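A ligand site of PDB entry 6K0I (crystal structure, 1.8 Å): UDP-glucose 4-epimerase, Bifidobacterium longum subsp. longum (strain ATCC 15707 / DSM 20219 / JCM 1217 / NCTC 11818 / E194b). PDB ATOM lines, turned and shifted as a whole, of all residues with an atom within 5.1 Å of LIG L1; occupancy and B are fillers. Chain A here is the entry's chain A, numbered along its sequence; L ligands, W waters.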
ATOM      1  N   LYS A  85     -15.603 -26.983   8.353  1.00  0.00           N
ATOM      2  CA  LYS A  85     -16.447 -26.975   9.544  1.00  0.00           C
ATOM      3  C   LYS A  85     -15.710 -26.917  10.909  1.00  0.00           C
ATOM      4  O   LYS A  85     -16.396 -27.092  11.947  1.00  0.00           O
ATOM      5  CB  LYS A  85     -17.332 -28.215   9.513  1.00  0.00           C
ATOM      6  CG  LYS A  85     -16.573 -29.519   9.652  1.00  0.00           C
ATOM      7  CD  LYS A  85     -17.370 -30.652  10.331  1.00  0.00           C
ATOM      8  CE  LYS A  85     -16.648 -31.973  10.245  1.00  0.00           C
ATOM      9  NZ  LYS A  85     -17.440 -33.052  10.902  1.00  0.00           N
ATOM     10  N   ALA A  86     -14.376 -26.709  10.966  1.00  0.00           N
ATOM     11  CA  ALA A  86     -13.689 -26.653  12.248  1.00  0.00           C
ATOM     12  C   ALA A  86     -13.551 -25.219  12.804  1.00  0.00           C
ATOM     13  O   ALA A  86     -12.861 -24.411  12.229  1.00  0.00           O
ATOM     14  CB  ALA A  86     -12.378 -27.287  12.082  1.00  0.00           C
ATOM     15  N   VAL A  87     -14.248 -24.947  13.901  1.00  0.00           N
ATOM     16  CA  VAL A  87     -14.203 -23.626  14.593  1.00  0.00           C
ATOM     17  C   VAL A  87     -12.746 -23.159  14.773  1.00  0.00           C
ATOM     18  O   VAL A  87     -12.402 -22.029  14.380  1.00  0.00           O
ATOM     19  CB  VAL A  87     -14.928 -23.736  15.941  1.00  0.00           C
ATOM     20  CG1 VAL A  87     -14.524 -22.616  16.881  1.00  0.00           C
ATOM     21  CG2 VAL A  87     -16.410 -23.770  15.736  1.00  0.00           C
ATOM     22  N   SER A 125     -25.886 -23.970  11.745  1.00  0.00           N
ATOM     23  CA  SER A 125     -25.041 -24.347  12.888  1.00  0.00           C
ATOM     24  C   SER A 125     -25.483 -23.563  14.121  1.00  0.00           C
ATOM     25  O   SER A 125     -25.778 -22.374  14.040  1.00  0.00           O
ATOM     26  CB  SER A 125     -23.594 -24.039  12.622  1.00  0.00           C
ATOM     27  OG  SER A 125     -22.765 -24.228  13.745  1.00  0.00           O
ATOM     28  N   ALA A 126     -25.492 -24.198  15.291  1.00  0.00           N
ATOM     29  CA  ALA A 126     -25.605 -23.490  16.572  1.00  0.00           C
ATOM     30  C   ALA A 126     -24.563 -22.348  16.721  1.00  0.00           C
ATOM     31  O   ALA A 126     -24.769 -21.471  17.548  1.00  0.00           O
ATOM     32  CB  ALA A 126     -25.414 -24.459  17.734  1.00  0.00           C
ATOM     33  N   THR A 127     -23.463 -22.385  15.939  1.00  0.00           N
ATOM     34  CA  THR A 127     -22.409 -21.340  16.054  1.00  0.00           C
ATOM     35  C   THR A 127     -22.970 -19.957  15.665  1.00  0.00           C
ATOM     36  O   THR A 127     -22.403 -18.896  16.053  1.00  0.00           O
ATOM     37  CB  THR A 127     -21.131 -21.687  15.256  1.00  0.00           C
ATOM     38  OG1 THR A 127     -21.515 -21.818  13.889  1.00  0.00           O
ATOM     39  CG2 THR A 127     -20.439 -22.904  15.814  1.00  0.00           C
ATOM     40  N   TYR A 150     -15.781 -19.615  10.971  1.00  0.00           N
ATOM     41  CA  TYR A 150     -16.710 -20.650  10.542  1.00  0.00           C
ATOM     42  C   TYR A 150     -18.174 -20.227  10.813  1.00  0.00           C
ATOM     43  O   TYR A 150     -19.038 -20.309   9.923  1.00  0.00           O
ATOM     44  CB  TYR A 150     -16.335 -21.982  11.226  1.00  0.00           C
ATOM     45  CG  TYR A 150     -17.453 -22.984  11.121  1.00  0.00           C
ATOM     46  CD1 TYR A 150     -17.801 -23.574   9.914  1.00  0.00           C
ATOM     47  CD2 TYR A 150     -18.208 -23.294  12.245  1.00  0.00           C
ATOM     48  CE1 TYR A 150     -18.867 -24.465   9.822  1.00  0.00           C
ATOM     49  CE2 TYR A 150     -19.276 -24.194  12.167  1.00  0.00           C
ATOM     50  CZ  TYR A 150     -19.574 -24.804  10.969  1.00  0.00           C
ATOM     51  OH  TYR A 150     -20.633 -25.733  10.895  1.00  0.00           O
ATOM     52  N   TYR A 178     -27.952 -27.207  12.972  1.00  0.00           N
ATOM     53  CA  TYR A 178     -27.569 -28.393  13.702  1.00  0.00           C
ATOM     54  C   TYR A 178     -26.782 -28.011  14.948  1.00  0.00           C
ATOM     55  O   TYR A 178     -26.014 -27.037  14.934  1.00  0.00           O
ATOM     56  CB  TYR A 178     -26.683 -29.349  12.901  1.00  0.00           C
ATOM     57  CG  TYR A 178     -27.015 -29.550  11.447  1.00  0.00           C
ATOM     58  CD1 TYR A 178     -28.303 -29.521  10.949  1.00  0.00           C
ATOM     59  CD2 TYR A 178     -26.012 -29.884  10.571  1.00  0.00           C
ATOM     60  CE1 TYR A 178     -28.551 -29.703   9.599  1.00  0.00           C
ATOM     61  CE2 TYR A 178     -26.248 -30.099   9.217  1.00  0.00           C
ATOM     62  CZ  TYR A 178     -27.529 -30.013   8.733  1.00  0.00           C
ATOM     63  OH  TYR A 178     -27.733 -30.235   7.385  1.00  0.00           O
ATOM     64  N   PHE A 179     -26.950 -28.808  16.007  1.00  0.00           N
ATOM     65  CA  PHE A 179     -26.066 -28.752  17.168  1.00  0.00           C
ATOM     66  C   PHE A 179     -24.916 -29.729  16.885  1.00  0.00           C
ATOM     67  O   PHE A 179     -24.251 -29.587  15.851  1.00  0.00           O
ATOM     68  CB  PHE A 179     -26.911 -28.829  18.444  1.00  0.00           C
ATOM     69  CG  PHE A 179     -27.591 -27.522  18.724  1.00  0.00           C
ATOM     70  CD1 PHE A 179     -27.275 -26.766  19.842  1.00  0.00           C
ATOM     71  CD2 PHE A 179     -28.508 -27.020  17.813  1.00  0.00           C
ATOM     72  CE1 PHE A 179     -27.863 -25.529  20.053  1.00  0.00           C
ATOM     73  CE2 PHE A 179     -29.088 -25.787  18.030  1.00  0.00           C
ATOM     74  CZ  PHE A 179     -28.804 -25.069  19.161  1.00  0.00           C
ATOM     75  N   ASN A 180     -24.665 -30.745  17.703  1.00  0.00           N
ATOM     76  CA  ASN A 180     -23.375 -31.499  17.531  1.00  0.00           C
ATOM     77  C   ASN A 180     -23.639 -32.982  17.260  1.00  0.00           C
ATOM     78  O   ASN A 180     -23.691 -33.801  18.180  1.00  0.00           O
ATOM     79  CB  ASN A 180     -22.456 -31.350  18.752  1.00  0.00           C
ATOM     80  CG  ASN A 180     -21.848 -29.952  18.891  1.00  0.00           C
ATOM     81  OD1 ASN A 180     -22.598 -28.977  18.938  1.00  0.00           O
ATOM     82  ND2 ASN A 180     -20.521 -29.894  19.048  1.00  0.00           N
ATOM     83  N   ALA A 199     -10.831 -33.278  13.889  1.00  0.00           N
ATOM     84  CA  ALA A 199     -10.994 -32.006  14.550  1.00  0.00           C
ATOM     85  C   ALA A 199     -12.171 -32.024  15.545  1.00  0.00           C
ATOM     86  O   ALA A 199     -12.212 -31.231  16.548  1.00  0.00           O
ATOM     87  CB  ALA A 199     -11.219 -30.931  13.479  1.00  0.00           C
ATOM     88  N   ASN A 200     -13.156 -32.888  15.325  1.00  0.00           N
ATOM     89  CA  ASN A 200     -14.283 -32.983  16.247  1.00  0.00           C
ATOM     90  C   ASN A 200     -13.957 -33.929  17.428  1.00  0.00           C
ATOM     91  O   ASN A 200     -13.097 -34.825  17.328  1.00  0.00           O
ATOM     92  CB  ASN A 200     -15.554 -33.430  15.490  1.00  0.00           C
ATOM     93  CG  ASN A 200     -16.077 -32.335  14.566  1.00  0.00           C
ATOM     94  OD1 ASN A 200     -15.793 -32.363  13.366  1.00  0.00           O
ATOM     95  ND2 ASN A 200     -16.732 -31.316  15.152  1.00  0.00           N
ATOM     96  N   LEU A 201     -14.659 -33.736  18.546  1.00  0.00           N
ATOM     97  CA  LEU A 201     -14.355 -34.443  19.791  1.00  0.00           C
ATOM     98  C   LEU A 201     -14.546 -35.946  19.647  1.00  0.00           C
ATOM     99  O   LEU A 201     -13.665 -36.733  19.938  1.00  0.00           O
ATOM    100  CB  LEU A 201     -15.241 -33.878  20.907  1.00  0.00           C
ATOM    101  CG  LEU A 201     -15.108 -34.621  22.229  1.00  0.00           C
ATOM    102  CD1 LEU A 201     -13.697 -34.516  22.810  1.00  0.00           C
ATOM    103  CD2 LEU A 201     -16.144 -34.107  23.213  1.00  0.00           C
ATOM    104  N   THR A 202     -15.742 -36.366  19.200  1.00  0.00           N
ATOM    105  CA  THR A 202     -16.087 -37.801  19.358  1.00  0.00           C
ATOM    106  C   THR A 202     -15.300 -38.701  18.402  1.00  0.00           C
ATOM    107  O   THR A 202     -14.917 -39.770  18.829  1.00  0.00           O
ATOM    108  CB  THR A 202     -17.601 -38.040  19.359  1.00  0.00           C
ATOM    109  OG1 THR A 202     -18.151 -37.753  18.075  1.00  0.00           O
ATOM    110  CG2 THR A 202     -18.287 -37.227  20.427  1.00  0.00           C
ATOM    111  N   TYR A 204     -12.256 -38.310  17.621  1.00  0.00           N
ATOM    112  CA  TYR A 204     -10.962 -38.358  18.285  1.00  0.00           C
ATOM    113  C   TYR A 204     -11.049 -39.322  19.479  1.00  0.00           C
ATOM    114  O   TYR A 204     -10.213 -40.268  19.617  1.00  0.00           O
ATOM    115  CB  TYR A 204     -10.512 -36.944  18.676  1.00  0.00           C
ATOM    116  CG  TYR A 204      -9.037 -36.822  18.957  1.00  0.00           C
ATOM    117  CD1 TYR A 204      -8.442 -37.516  20.014  1.00  0.00           C
ATOM    118  CD2 TYR A 204      -8.231 -35.977  18.231  1.00  0.00           C
ATOM    119  CE1 TYR A 204      -7.080 -37.445  20.264  1.00  0.00           C
ATOM    120  CE2 TYR A 204      -6.882 -35.874  18.485  1.00  0.00           C
ATOM    121  CZ  TYR A 204      -6.309 -36.568  19.518  1.00  0.00           C
ATOM    122  OH  TYR A 204      -4.976 -36.407  19.763  1.00  0.00           O
ATOM    123  N   GLN A 217      -7.387 -34.758  23.895  1.00  0.00           N
ATOM    124  CA  GLN A 217      -6.937 -33.403  24.204  1.00  0.00           C
ATOM    125  C   GLN A 217      -8.169 -32.595  24.619  1.00  0.00           C
ATOM    126  O   GLN A 217      -9.020 -32.405  23.770  1.00  0.00           O
ATOM    127  CB  GLN A 217      -6.262 -32.755  22.965  1.00  0.00           C
ATOM    128  CG  GLN A 217      -5.209 -33.640  22.344  1.00  0.00           C
ATOM    129  CD  GLN A 217      -4.022 -33.850  23.255  1.00  0.00           C
ATOM    130  OE1 GLN A 217      -3.278 -32.879  23.553  1.00  0.00           O
ATOM    131  NE2 GLN A 217      -3.876 -35.066  23.765  1.00  0.00           N
ATOM    132  N   VAL A 218      -8.321 -32.257  25.912  1.00  0.00           N
ATOM    133  CA  VAL A 218      -9.509 -31.535  26.350  1.00  0.00           C
ATOM    134  C   VAL A 218      -9.188 -30.044  26.323  1.00  0.00           C
ATOM    135  O   VAL A 218      -8.280 -29.600  27.075  1.00  0.00           O
ATOM    136  CB  VAL A 218      -9.966 -31.967  27.753  1.00  0.00           C
ATOM    137  CG1 VAL A 218     -11.127 -31.146  28.268  1.00  0.00           C
ATOM    138  CG2 VAL A 218     -10.279 -33.445  27.742  1.00  0.00           C
ATOM    139  N   TYR A 219      -9.862 -29.288  25.441  1.00  0.00           N
ATOM    140  CA  TYR A 219      -9.492 -27.906  25.187  1.00  0.00           C
ATOM    141  C   TYR A 219     -10.145 -26.980  26.184  1.00  0.00           C
ATOM    142  O   TYR A 219     -11.257 -26.502  25.955  1.00  0.00           O
ATOM    143  CB  TYR A 219      -9.811 -27.539  23.740  1.00  0.00           C
ATOM    144  CG  TYR A 219      -9.053 -28.355  22.720  1.00  0.00           C
ATOM    145  CD1 TYR A 219      -7.686 -28.570  22.836  1.00  0.00           C
ATOM    146  CD2 TYR A 219      -9.728 -28.875  21.625  1.00  0.00           C
ATOM    147  CE1 TYR A 219      -6.992 -29.313  21.885  1.00  0.00           C
ATOM    148  CE2 TYR A 219      -9.048 -29.610  20.663  1.00  0.00           C
ATOM    149  CZ  TYR A 219      -7.707 -29.850  20.814  1.00  0.00           C
ATOM    150  OH  TYR A 219      -7.075 -30.587  19.879  1.00  0.00           O
ATOM    151  N   GLY A 230     -16.169 -27.526  27.934  1.00  0.00           N
ATOM    152  CA  GLY A 230     -17.268 -27.152  27.065  1.00  0.00           C
ATOM    153  C   GLY A 230     -18.474 -28.058  27.174  1.00  0.00           C
ATOM    154  O   GLY A 230     -18.305 -29.304  27.291  1.00  0.00           O
ATOM    155  N   VAL A 231     -19.673 -27.445  27.094  1.00  0.00           N
ATOM    156  CA  VAL A 231     -20.942 -28.159  27.064  1.00  0.00           C
ATOM    157  C   VAL A 231     -21.600 -27.994  25.686  1.00  0.00           C
ATOM    158  O   VAL A 231     -21.735 -26.883  25.156  1.00  0.00           O
ATOM    159  CB  VAL A 231     -21.866 -27.673  28.209  1.00  0.00           C
ATOM    160  CG1 VAL A 231     -23.312 -28.146  28.048  1.00  0.00           C
ATOM    161  CG2 VAL A 231     -21.280 -28.084  29.553  1.00  0.00           C
ATOM    162  N   ARG A 232     -22.081 -29.106  25.159  1.00  0.00           N
ATOM    163  CA  ARG A 232     -22.703 -29.122  23.855  1.00  0.00           C
ATOM    164  C   ARG A 232     -23.906 -30.062  23.897  1.00  0.00           C
ATOM    165  O   ARG A 232     -24.011 -30.989  24.732  1.00  0.00           O
ATOM    166  CB  ARG A 232     -21.712 -29.605  22.788  1.00  0.00           C
ATOM    167  CG  ARG A 232     -20.440 -28.758  22.653  1.00  0.00           C
ATOM    168  CD  ARG A 232     -20.727 -27.391  22.044  1.00  0.00           C
ATOM    169  NE  ARG A 232     -19.481 -26.651  21.789  1.00  0.00           N
ATOM    170  CZ  ARG A 232     -18.903 -25.777  22.634  1.00  0.00           C
ATOM    171  NH1 ARG A 232     -19.387 -25.615  23.858  1.00  0.00           N
ATOM    172  NH2 ARG A 232     -17.840 -25.065  22.256  1.00  0.00           N
ATOM    173  N   TYR A 234     -25.235 -32.877  21.997  1.00  0.00           N
ATOM    174  CA  TYR A 234     -24.917 -33.929  21.122  1.00  0.00           C
ATOM    175  C   TYR A 234     -26.233 -34.567  20.618  1.00  0.00           C
ATOM    176  O   TYR A 234     -27.170 -34.791  21.403  1.00  0.00           O
ATOM    177  CB  TYR A 234     -23.951 -34.940  21.779  1.00  0.00           C
ATOM    178  CG  TYR A 234     -22.619 -34.285  22.127  1.00  0.00           C
ATOM    179  CD1 TYR A 234     -21.713 -33.972  21.134  1.00  0.00           C
ATOM    180  CD2 TYR A 234     -22.349 -33.817  23.386  1.00  0.00           C
ATOM    181  CE1 TYR A 234     -20.536 -33.300  21.389  1.00  0.00           C
ATOM    182  CE2 TYR A 234     -21.160 -33.159  23.689  1.00  0.00           C
ATOM    183  CZ  TYR A 234     -20.258 -32.882  22.674  1.00  0.00           C
ATOM    184  OH  TYR A 234     -19.081 -32.205  22.878  1.00  0.00           O
ATOM    185  N   VAL A 269     -17.365 -32.049  27.961  1.00  0.00           N
ATOM    186  CA  VAL A 269     -16.366 -32.890  27.318  1.00  0.00           C
ATOM    187  C   VAL A 269     -16.078 -34.140  28.186  1.00  0.00           C
ATOM    188  O   VAL A 269     -15.915 -35.246  27.690  1.00  0.00           O
ATOM    189  CB  VAL A 269     -15.084 -32.094  27.020  1.00  0.00           C
ATOM    190  CG1 VAL A 269     -14.031 -33.001  26.420  1.00  0.00           C
ATOM    191  CG2 VAL A 269     -15.361 -30.907  26.089  1.00  0.00           C
ATOM    192  N   ARG A 292      -9.169 -23.893  22.868  1.00  0.00           N
ATOM    193  CA  ARG A 292      -9.067 -23.774  21.433  1.00  0.00           C
ATOM    194  C   ARG A 292      -9.697 -22.446  21.023  1.00  0.00           C
ATOM    195  O   ARG A 292     -10.820 -22.082  21.435  1.00  0.00           O
ATOM    196  CB  ARG A 292      -9.743 -24.971  20.755  1.00  0.00           C
ATOM    197  CG  ARG A 292      -9.663 -24.980  19.234  1.00  0.00           C
ATOM    198  CD  ARG A 292     -10.241 -26.309  18.768  1.00  0.00           C
ATOM    199  NE  ARG A 292     -11.692 -26.321  18.986  1.00  0.00           N
ATOM    200  CZ  ARG A 292     -12.528 -27.326  18.696  1.00  0.00           C
ATOM    201  NH1 ARG A 292     -12.063 -28.441  18.169  1.00  0.00           N
ATOM    202  NH2 ARG A 292     -13.832 -27.180  18.926  1.00  0.00           N
ATOM    203  N   ASP A 295     -13.923 -21.322  20.618  1.00  0.00           N
ATOM    204  CA  ASP A 295     -14.888 -22.143  21.377  1.00  0.00           C
ATOM    205  C   ASP A 295     -15.599 -21.281  22.423  1.00  0.00           C
ATOM    206  O   ASP A 295     -14.960 -20.424  23.078  1.00  0.00           O
ATOM    207  CB  ASP A 295     -14.239 -23.311  22.108  1.00  0.00           C
ATOM    208  CG  ASP A 295     -13.718 -24.424  21.225  1.00  0.00           C
ATOM    209  OD1 ASP A 295     -14.123 -24.475  20.004  1.00  0.00           O
ATOM    210  OD2 ASP A 295     -12.980 -25.298  21.796  1.00  0.00           O
ATOM    211  N   ILE A 296     -16.891 -21.567  22.623  1.00  0.00           N
ATOM    212  CA  ILE A 296     -17.683 -20.977  23.666  1.00  0.00           C
ATOM    213  C   ILE A 296     -17.923 -22.038  24.735  1.00  0.00           C
ATOM    214  O   ILE A 296     -17.663 -23.211  24.577  1.00  0.00           O
ATOM    215  CB  ILE A 296     -19.013 -20.432  23.136  1.00  0.00           C
ATOM    216  CG1 ILE A 296     -19.836 -21.555  22.474  1.00  0.00           C
ATOM    217  CG2 ILE A 296     -18.708 -19.276  22.199  1.00  0.00           C
ATOM    218  CD1 ILE A 296     -21.303 -21.446  22.619  1.00  0.00           C
ATOM    219  N   CYS A 299     -23.701 -24.506  24.742  1.00  0.00           N
ATOM    220  CA  CYS A 299     -24.848 -24.302  23.901  1.00  0.00           C
ATOM    221  C   CYS A 299     -25.628 -25.620  23.798  1.00  0.00           C
ATOM    222  O   CYS A 299     -25.051 -26.690  23.711  1.00  0.00           O
ATOM    223  CB  CYS A 299     -24.516 -23.763  22.510  1.00  0.00           C
ATOM    224  SG  CYS A 299     -23.389 -24.823  21.559  1.00  0.00           S
HETATM  225  N1  LIG L   1     -13.137 -30.536  22.158  1.00  0.00           N
HETATM  226  C1  LIG L   1     -12.088 -31.053  22.876  1.00  0.00           C
HETATM  227  N2  LIG L   1     -11.195 -31.827  22.225  1.00  0.00           N
HETATM  228  C2  LIG L   1     -11.233 -32.076  20.944  1.00  0.00           C
HETATM  229  C3  LIG L   1     -12.270 -31.525  20.182  1.00  0.00           C
HETATM  230  C4  LIG L   1     -13.205 -30.785  20.827  1.00  0.00           C
HETATM  231  O1  LIG L   1     -12.010 -30.822  24.124  1.00  0.00           O
HETATM  232  O2  LIG L   1     -10.341 -32.782  20.441  1.00  0.00           O
HETATM  233  C5  LIG L   1     -14.198 -29.811  22.798  1.00  0.00           C
HETATM  234  C6  LIG L   1     -14.492 -28.427  22.286  1.00  0.00           C
HETATM  235  O3  LIG L   1     -13.770 -27.483  23.098  1.00  0.00           O
HETATM  236  C7  LIG L   1     -16.009 -28.365  22.464  1.00  0.00           C
HETATM  237  C8  LIG L   1     -16.516 -29.785  22.298  1.00  0.00           C
HETATM  238  O4  LIG L   1     -15.405 -30.615  22.576  1.00  0.00           O
HETATM  239  O5  LIG L   1     -16.333 -27.900  23.774  1.00  0.00           O
HETATM  240  C9  LIG L   1     -17.097 -30.018  20.919  1.00  0.00           C
HETATM  241  O6  LIG L   1     -16.077 -29.651  19.980  1.00  0.00           O
HETATM  242  P1  LIG L   1     -16.182 -30.048  18.435  1.00  0.00           P
HETATM  243  O7  LIG L   1     -14.866 -29.543  17.827  1.00  0.00           O
HETATM  244  O8  LIG L   1     -16.548 -31.504  18.233  1.00  0.00           O
HETATM  245  O9  LIG L   1     -17.449 -29.293  17.997  1.00  0.00           O
HETATM  246  P2  LIG L   1     -17.871 -27.715  18.053  1.00  0.00           P
HETATM  247  O10 LIG L   1     -18.848 -27.426  19.177  1.00  0.00           O
HETATM  248  O11 LIG L   1     -16.703 -26.810  17.939  1.00  0.00           O
HETATM  249  O12 LIG L   1     -18.516 -27.522  16.586  1.00  0.00           O
HETATM  250  C10 LIG L   1     -19.282 -28.604  15.970  1.00  0.00           C
HETATM  251  C11 LIG L   1     -18.914 -28.687  14.500  1.00  0.00           C
HETATM  252  C12 LIG L   1     -19.380 -27.463  13.821  1.00  0.00           C
HETATM  253  C13 LIG L   1     -20.857 -27.233  14.111  1.00  0.00           C
HETATM  254  C14 LIG L   1     -21.149 -27.016  15.617  1.00  0.00           C
HETATM  255  C15 LIG L   1     -22.663 -26.777  15.873  1.00  0.00           C
HETATM  256  O13 LIG L   1     -17.483 -28.822  14.158  1.00  0.00           O
HETATM  257  O14 LIG L   1     -19.223 -27.645  12.378  1.00  0.00           O
HETATM  258  O15 LIG L   1     -21.333 -26.138  13.328  1.00  0.00           O
HETATM  259  O16 LIG L   1     -20.670 -28.229  16.250  1.00  0.00           O
HETATM  260  O17 LIG L   1     -22.632 -26.657  17.326  1.00  0.00           O
HETATM  261  P1  LG2 L   2     -17.893 -33.342   6.590  1.00  0.00           P
HETATM  262  O1  LG2 L   2     -16.568 -32.670   6.474  1.00  0.00           O
HETATM  263  O2  LG2 L   2     -17.862 -34.823   6.888  1.00  0.00           O
HETATM  264  O3  LG2 L   2     -18.788 -33.129   5.316  1.00  0.00           O
HETATM  265  C1  LG2 L   2     -18.705 -32.025   4.440  1.00  0.00           C
HETATM  266  C2  LG2 L   2     -18.300 -32.569   3.108  1.00  0.00           C
HETATM  267  O4  LG2 L   2     -18.197 -31.481   2.117  1.00  0.00           O
HETATM  268  C3  LG2 L   2     -17.014 -33.410   2.985  1.00  0.00           C
HETATM  269  O5  LG2 L   2     -17.269 -34.681   2.361  1.00  0.00           O
HETATM  270  C4  LG2 L   2     -16.091 -32.549   2.128  1.00  0.00           C
HETATM  271  O6  LG2 L   2     -15.170 -33.219   1.313  1.00  0.00           O
HETATM  272  C5  LG2 L   2     -17.118 -31.787   1.289  1.00  0.00           C
HETATM  273  N1  LG2 L   2     -16.737 -30.481   0.776  1.00  0.00           N
HETATM  274  C6  LG2 L   2     -16.322 -29.407   1.514  1.00  0.00           C
HETATM  275  N2  LG2 L   2     -16.173 -28.312   0.709  1.00  0.00           N
HETATM  276  C7  LG2 L   2     -16.474 -28.736  -0.548  1.00  0.00           C
HETATM  277  C8  LG2 L   2     -16.536 -28.144  -1.841  1.00  0.00           C
HETATM  278  N3  LG2 L   2     -16.180 -26.844  -1.969  1.00  0.00           N
HETATM  279  N4  LG2 L   2     -16.962 -28.847  -2.916  1.00  0.00           N
HETATM  280  C9  LG2 L   2     -17.253 -30.129  -2.788  1.00  0.00           C
HETATM  281  N5  LG2 L   2     -17.250 -30.750  -1.642  1.00  0.00           N
HETATM  282  C10 LG2 L   2     -16.861 -30.132  -0.487  1.00  0.00           C
HETATM  283  O7  LG2 L   2     -18.682 -32.599   7.710  1.00  0.00           O
HETATM  284  P2  LG2 L   2     -20.132 -32.880   8.357  1.00  0.00           P
HETATM  285  O8  LG2 L   2     -20.851 -33.867   7.506  1.00  0.00           O
HETATM  286  O9  LG2 L   2     -19.904 -33.062   9.847  1.00  0.00           O
HETATM  287  O10 LG2 L   2     -20.881 -31.468   8.176  1.00  0.00           O
HETATM  288  C11 LG2 L   2     -21.606 -31.189   6.979  1.00  0.00           C
HETATM  289  C12 LG2 L   2     -22.189 -29.810   7.010  1.00  0.00           C
HETATM  290  O11 LG2 L   2     -22.882 -29.602   8.185  1.00  0.00           O
HETATM  291  C13 LG2 L   2     -21.129 -28.690   6.987  1.00  0.00           C
HETATM  292  O12 LG2 L   2     -21.523 -27.539   6.208  1.00  0.00           O
HETATM  293  C14 LG2 L   2     -20.997 -28.295   8.380  1.00  0.00           C
HETATM  294  O13 LG2 L   2     -20.522 -26.947   8.573  1.00  0.00           O
HETATM  295  C15 LG2 L   2     -22.398 -28.456   8.902  1.00  0.00           C
HETATM  296  N6  LG2 L   2     -22.484 -28.717  10.336  1.00  0.00           N
HETATM  297  C16 LG2 L   2     -21.841 -29.732  10.912  1.00  0.00           C
HETATM  298  C17 LG2 L   2     -22.050 -29.964  12.239  1.00  0.00           C
HETATM  299  C18 LG2 L   2     -21.255 -31.090  12.913  1.00  0.00           C
HETATM  300  O14 LG2 L   2     -20.585 -31.964  12.306  1.00  0.00           O
HETATM  301  N7  LG2 L   2     -21.166 -31.006  14.183  1.00  0.00           N
HETATM  302  C19 LG2 L   2     -22.942 -29.160  12.949  1.00  0.00           C
HETATM  303  C20 LG2 L   2     -23.592 -28.098  12.325  1.00  0.00           C
HETATM  304  C21 LG2 L   2     -23.349 -27.935  11.009  1.00  0.00           C
HETATM  305  O   HOH W   1     -21.010 -25.342  18.846  1.00  0.00           O
HETATM  306  O   HOH W   2     -16.753 -24.753  19.572  1.00  0.00           O
HETATM  307  O   HOH W   3     -13.936 -27.317  26.131  1.00  0.00           O
HETATM  308  O   HOH W   4      -9.172 -32.289  17.896  1.00  0.00           O
HETATM  309  O   HOH W   5     -14.543 -29.995  12.729  1.00  0.00           O
HETATM  310  O   HOH W   6      -8.770 -34.795  21.400  1.00  0.00           O
HETATM  311  O   HOH W   7     -13.742 -28.891  15.166  1.00  0.00           O
HETATM  312  O   HOH W   8     -15.689 -27.096  15.364  1.00  0.00           O
HETATM  313  O   HOH W   9     -15.626 -25.197  24.745  1.00  0.00           O
HETATM  314  O   HOH W  10     -19.062 -32.313  18.259  1.00  0.00           O
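The side-chain hydroxyl (OG) of Ser 125 sits at hydrogen-bond distance from an oxygen (O15) of LIG L1 (2.4 Å).
The side-chain hydroxyl of Tyr 150 lies within hydrogen-bond range of an oxygen (O15) of LIG L1, at 2.6 Å.
The side-chain carboxylate of Asp 295 lies within hydrogen-bond range of an oxygen (O3) of LIG L1 (2.7 Å).
The backbone carbonyl oxygen (O) of Gln 217 lies within hydrogen-bond range of a nitrogen (N2) of LIG L1 (2.7 Å).
ND2 of Asn 200 is in hydrogen-bond range of O13 of LIG L1 (2.8 Å).
An oxygen (O10) of LIG L1 is in salt-bridge range of the guanidinium group of Arg 232 (2.8 Å).
The guanidinium group (NH2) of Arg 292 is in salt-bridge range of an oxygen (O7) of LIG L1 (2.8 Å).
An oxygen (O17) of LIG L1 lies within hydrogen-bond range of the side-chain amide oxygen (OD1) of Asn 180.
An oxygen (O14) of LIG L1 lies within hydrogen-bond range of the backbone carbonyl oxygen (O) of Lys 85 (2.9 Å).
The backbone NH (N) of Leu 201 sits at hydrogen-bond distance from an oxygen (O8) of LIG L1.
The backbone NH of Tyr 219 is in hydrogen-bond range of an oxygen (O1) of LIG L1.
An oxygen (O13) of LG2 L2 sits at hydrogen-bond distance from the side-chain hydroxyl of Tyr 150 (2.6 Å).
NZ of Lys 85 lies within salt-bridge range of O9 of LG2 L2.
A nitrogen (N7) of LG2 L2 lies close to an oxygen (O16) of LIG L1 (3.5 Å).
OG of Ser 125 sits at hydrogen-bond distance from OG1 of Thr 127.
The side-chain carboxylate (OD1) of Asp 295 lies within salt-bridge range of the guanidinium group (NH2) of Arg 292.
The side-chain amide oxygen (OD1) of Asn 200 lies within hydrogen-bond range of the side-chain amino group (NZ) of Lys 85 (3.0 Å).
The backbone carbonyl oxygen of Ile 296 lies within hydrogen-bond range of the guanidinium group of Arg 232, at 3.0 Å.
The backbone carbonyl oxygen (O) of Ala 199 lies within hydrogen-bond range of the guanidinium group (NH1) of Arg 292 (3.2 Å).
O of Tyr 178 lies within hydrogen-bond range of N of Ala 126, at 2.9 Å.
The backbone NH of Val 269 lies within hydrogen-bond range of the backbone carbonyl oxygen of Gly 230 (3.0 Å).
O of Ala 199 sits close to O7 of LIG L1, at 3.4 Å.
Residues that only touch LIG L1: Val 87, Ala 126, Tyr 178, Phe 179, Val 218, Gly 230, Tyr 234 and Val 269.
Hydrophobic or aromatic side chains within 4 Å of LIG L1: Val 87, Ala 126, Tyr 150, Leu 201, Tyr 219 and Val 269.
20 residues have an atom within 4 Å of LIG L1: Lys 85, Val 87, Ser 125, Ala 126, Tyr 150, Tyr 178, Phe 179, Asn 180, Ala 199, Asn 200, Leu 201, Gln 217, Val 218, Tyr 219, Gly 230, Arg 232, Tyr 234, Val 269, Arg 292 and Asp 295.
Water W1 bridges O17 of LIG L1 (2.6 Å) and SG of Cys 299 (3.6 Å).
Water W2 lies within hydrogen-bond range of O11 of LIG L1 (2.6 Å), OD1 of Asp 295 (2.7 Å) and NH2 of Arg 232 (2.9 Å).
Water W8 lies within hydrogen-bond range of O13 of LIG L1 (2.8 Å), N of Val 87 (3.0 Å) and O of Lys 85 (3.5 Å).
Water W7 lies within hydrogen-bond range of O7 of LIG L1, O of Ala 199 and NH1 of Arg 292.
Water W3 lies within hydrogen-bond range of the backbone carbonyl oxygen of Tyr 219, the backbone NH of Gly 230 and an oxygen (O3) of LIG L1.
Water W5 lies within hydrogen-bond range of the side-chain amide oxygen of Asn 200 and an oxygen (O13) of LIG L1.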
